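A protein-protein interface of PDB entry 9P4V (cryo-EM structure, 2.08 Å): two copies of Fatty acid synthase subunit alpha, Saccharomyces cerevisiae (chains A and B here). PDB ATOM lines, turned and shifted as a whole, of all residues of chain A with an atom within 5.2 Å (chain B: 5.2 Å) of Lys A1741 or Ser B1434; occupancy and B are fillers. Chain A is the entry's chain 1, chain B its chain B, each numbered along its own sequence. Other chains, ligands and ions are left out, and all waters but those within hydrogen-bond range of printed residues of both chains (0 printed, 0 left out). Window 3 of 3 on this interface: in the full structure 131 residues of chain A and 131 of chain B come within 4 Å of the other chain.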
ATOM      1  N   GLN A1739      -6.788  21.185 -18.823  1.00  0.00           N
ATOM      2  CA  GLN A1739      -7.079  22.299 -17.919  1.00  0.00           C
ATOM      3  C   GLN A1739      -6.753  23.639 -18.581  1.00  0.00           C
ATOM      4  O   GLN A1739      -6.116  24.512 -17.991  1.00  0.00           O
ATOM      5  CB  GLN A1739      -6.330  22.140 -16.594  1.00  0.00           C
ATOM      6  CG  GLN A1739      -6.656  20.858 -15.839  1.00  0.00           C
ATOM      7  CD  GLN A1739      -8.008  20.895 -15.146  1.00  0.00           C
ATOM      8  OE1 GLN A1739      -8.683  21.919 -15.133  1.00  0.00           O
ATOM      9  NE2 GLN A1739      -8.402  19.772 -14.563  1.00  0.00           N
ATOM     10  N   SER A1740      -7.211  23.802 -19.818  1.00  0.00           N
ATOM     11  CA  SER A1740      -6.926  24.984 -20.615  1.00  0.00           C
ATOM     12  C   SER A1740      -8.161  25.868 -20.726  1.00  0.00           C
ATOM     13  O   SER A1740      -9.296  25.386 -20.735  1.00  0.00           O
ATOM     14  CB  SER A1740      -6.438  24.599 -22.013  1.00  0.00           C
ATOM     15  OG  SER A1740      -7.382  23.785 -22.680  1.00  0.00           O
ATOM     16  N   LYS A1741      -7.924  27.176 -20.812  1.00  0.00           N
ATOM     17  CA  LYS A1741      -9.025  28.122 -20.959  1.00  0.00           C
ATOM     18  C   LYS A1741      -9.765  27.924 -22.276  1.00  0.00           C
ATOM     19  O   LYS A1741     -10.955  28.247 -22.373  1.00  0.00           O
ATOM     20  CB  LYS A1741      -8.500  29.552 -20.860  1.00  0.00           C
ATOM     21  N   ASP A1742      -9.081  27.404 -23.297  1.00  0.00           N
ATOM     22  CA  ASP A1742      -9.713  27.231 -24.601  1.00  0.00           C
ATOM     23  C   ASP A1742     -10.854  26.224 -24.538  1.00  0.00           C
ATOM     24  O   ASP A1742     -11.922  26.446 -25.120  1.00  0.00           O
ATOM     25  CB  ASP A1742      -8.670  26.792 -25.626  1.00  0.00           C
ATOM     26  N   SER A1743     -10.651  25.115 -23.837  1.00  0.00           N
ATOM     27  CA  SER A1743     -11.681  24.087 -23.736  1.00  0.00           C
ATOM     28  C   SER A1743     -12.935  24.617 -23.065  1.00  0.00           C
ATOM     29  O   SER A1743     -14.045  24.303 -23.483  1.00  0.00           O
ATOM     30  CB  SER A1743     -11.134  22.907 -22.942  1.00  0.00           C
ATOM     31  OG  SER A1743      -9.949  22.405 -23.529  1.00  0.00           O
ATOM     32  N   TYR A1744     -12.766  25.427 -22.029  1.00  0.00           N
ATOM     33  CA  TYR A1744     -13.898  25.965 -21.293  1.00  0.00           C
ATOM     34  C   TYR A1744     -14.648  26.995 -22.126  1.00  0.00           C
ATOM     35  O   TYR A1744     -15.873  26.937 -22.236  1.00  0.00           O
ATOM     36  CB  TYR A1744     -13.430  26.586 -19.978  1.00  0.00           C
ATOM     37  CG  TYR A1744     -14.559  27.025 -19.080  1.00  0.00           C
ATOM     38  CD1 TYR A1744     -15.382  26.095 -18.459  1.00  0.00           C
ATOM     39  CD2 TYR A1744     -14.804  28.372 -18.847  1.00  0.00           C
ATOM     40  CE1 TYR A1744     -16.414  26.490 -17.638  1.00  0.00           C
ATOM     41  CE2 TYR A1744     -15.834  28.778 -18.022  1.00  0.00           C
ATOM     42  CZ  TYR A1744     -16.633  27.832 -17.417  1.00  0.00           C
ATOM     43  OH  TYR A1744     -17.665  28.226 -16.598  1.00  0.00           O
ATOM     44  N   HIS B1432     -12.969  21.020 -13.796  1.00  0.00           N
ATOM     45  CA  HIS B1432     -12.217  21.951 -14.625  1.00  0.00           C
ATOM     46  C   HIS B1432     -11.904  23.202 -13.817  1.00  0.00           C
ATOM     47  O   HIS B1432     -12.817  23.868 -13.322  1.00  0.00           O
ATOM     48  CB  HIS B1432     -13.005  22.304 -15.881  1.00  0.00           C
ATOM     49  CG  HIS B1432     -12.179  22.959 -16.937  1.00  0.00           C
ATOM     50  ND1 HIS B1432     -11.213  22.285 -17.649  1.00  0.00           N
ATOM     51  CD2 HIS B1432     -12.156  24.234 -17.385  1.00  0.00           C
ATOM     52  CE1 HIS B1432     -10.641  23.113 -18.502  1.00  0.00           C
ATOM     53  NE2 HIS B1432     -11.198  24.302 -18.363  1.00  0.00           N
ATOM     54  N   HIS B1433     -10.618  23.517 -13.682  1.00  0.00           N
ATOM     55  CA  HIS B1433     -10.163  24.627 -12.853  1.00  0.00           C
ATOM     56  C   HIS B1433      -9.502  25.736 -13.657  1.00  0.00           C
ATOM     57  O   HIS B1433      -8.939  26.658 -13.065  1.00  0.00           O
ATOM     58  CB  HIS B1433      -9.184  24.127 -11.788  1.00  0.00           C
ATOM     59  CG  HIS B1433      -9.810  23.237 -10.761  1.00  0.00           C
ATOM     60  ND1 HIS B1433      -9.150  22.163 -10.206  1.00  0.00           N
ATOM     61  CD2 HIS B1433     -11.035  23.264 -10.187  1.00  0.00           C
ATOM     62  CE1 HIS B1433      -9.944  21.562  -9.340  1.00  0.00           C
ATOM     63  NE2 HIS B1433     -11.091  22.214  -9.306  1.00  0.00           N
ATOM     64  N   SER B1434      -9.514  25.649 -14.980  1.00  0.00           N
ATOM     65  CA  SER B1434      -8.819  26.642 -15.792  1.00  0.00           C
ATOM     66  C   SER B1434      -9.307  28.025 -15.445  1.00  0.00           C
ATOM     67  O   SER B1434      -8.567  28.996 -15.576  1.00  0.00           O
ATOM     68  CB  SER B1434      -9.034  26.381 -17.281  1.00  0.00           C
ATOM     69  OG  SER B1434     -10.356  26.700 -17.675  1.00  0.00           O
ATOM     70  N   SER B1435     -10.554  28.117 -15.010  1.00  0.00           N
ATOM     71  CA  SER B1435     -11.129  29.392 -14.652  1.00  0.00           C
ATOM     72  C   SER B1435     -11.834  29.251 -13.325  1.00  0.00           C
ATOM     73  O   SER B1435     -12.948  28.735 -13.271  1.00  0.00           O
ATOM     74  CB  SER B1435     -12.114  29.823 -15.723  1.00  0.00           C
ATOM     75  OG  SER B1435     -11.465  29.977 -16.973  1.00  0.00           O
ATOM     76  N   VAL B1436     -11.195  29.703 -12.254  1.00  0.00           N
ATOM     77  CA  VAL B1436     -11.779  29.585 -10.924  1.00  0.00           C
ATOM     78  C   VAL B1436     -11.569  30.860 -10.116  1.00  0.00           C
ATOM     79  O   VAL B1436     -11.644  30.839  -8.889  1.00  0.00           O
ATOM     80  CB  VAL B1436     -11.172  28.388 -10.173  1.00  0.00           C
ATOM     81  CG1 VAL B1436     -11.479  27.096 -10.912  1.00  0.00           C
ATOM     82  CG2 VAL B1436      -9.670  28.557 -10.026  1.00  0.00           C
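Lys A1741 touches one residue of chain B. Of chain A, only Gln A1739, Ser A1740, Lys A1741 and Tyr A1744 come within 4 Å of Ser B1434. Printed residues of chain B within 4 Å of Ser A1740: His B1432 and Ser B1434. Of the printed residues of chain B, Tyr A1744 touches His B1432 and Ser B1434. Printed residues of chain B within 4 Å of Gln A1739: His B1432 (3.6 Å), His B1433 (2.9 Å) and Ser B1434 (3.5 Å). Of the printed residues of chain A, His B1432 touches Gln A1739 (3.6 Å), Ser A1740 (3.2 Å) and Tyr A1744 (3.6 Å). Printed residues of chain A within 4 Å of His B1433: Gln A1739 (2.9 Å). Asp A1742 touches none of the printed residues of chain B. Ser B1435 touches none of the printed residues of chain A. The nearest printed residue of chain A that does not touch His B1433 is Ser A1740 (6.9 Å).
NE2 of His B1432 sits at hydrogen-bond distance from O of Ser A1740 (3.2 Å). The side-chain hydroxyl (OG) of Ser B1434 lies within hydrogen-bond range of the backbone carbonyl oxygen (O) of Ser A1740. The side-chain amide oxygen (OE1) of Gln A1739 sits at hydrogen-bond distance from the backbone NH (N) of His B1433 (2.9 Å).
The side-chain hydroxyl (OG) of Ser A1740 lies within hydrogen-bond range of the side-chain hydroxyl (OG) of Ser A1743 (3.0 Å). A ring nitrogen (NE2) of His B1432 lies within hydrogen-bond range of the side-chain hydroxyl (OG) of Ser B1434 (2.6 Å).
Gln A1739 touches His B1432. O of Gln A1739 touches CB of Ser B1434, at 3.5 Å. Ser B1434 touches Lys A1741. His B1432 touches Tyr A1744 (NE2 to CB, 3.6 Å). OG of Ser B1434 touches CB of Tyr A1744, 3.8 Å away.
Printed residues of chain A that touch a printed residue of chain B: Gln A1739, Ser A1740, Lys A1741 and Tyr A1744. Of the 5 printed residues of chain B, 3 touch a printed residue of chain A. Printed residues of chain B that touch a printed residue of chain A: His B1432, His B1433 and Ser B1434. Among the printed residues, no Asp or Glu carboxylate lies within 4 Å of a Lys or Arg side-chain nitrogen of the other chain.
No position is printed for both chains. Of the 8 pairs that touch across the chains among the printed residues, none has its exchanged pair printed and touching as well.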
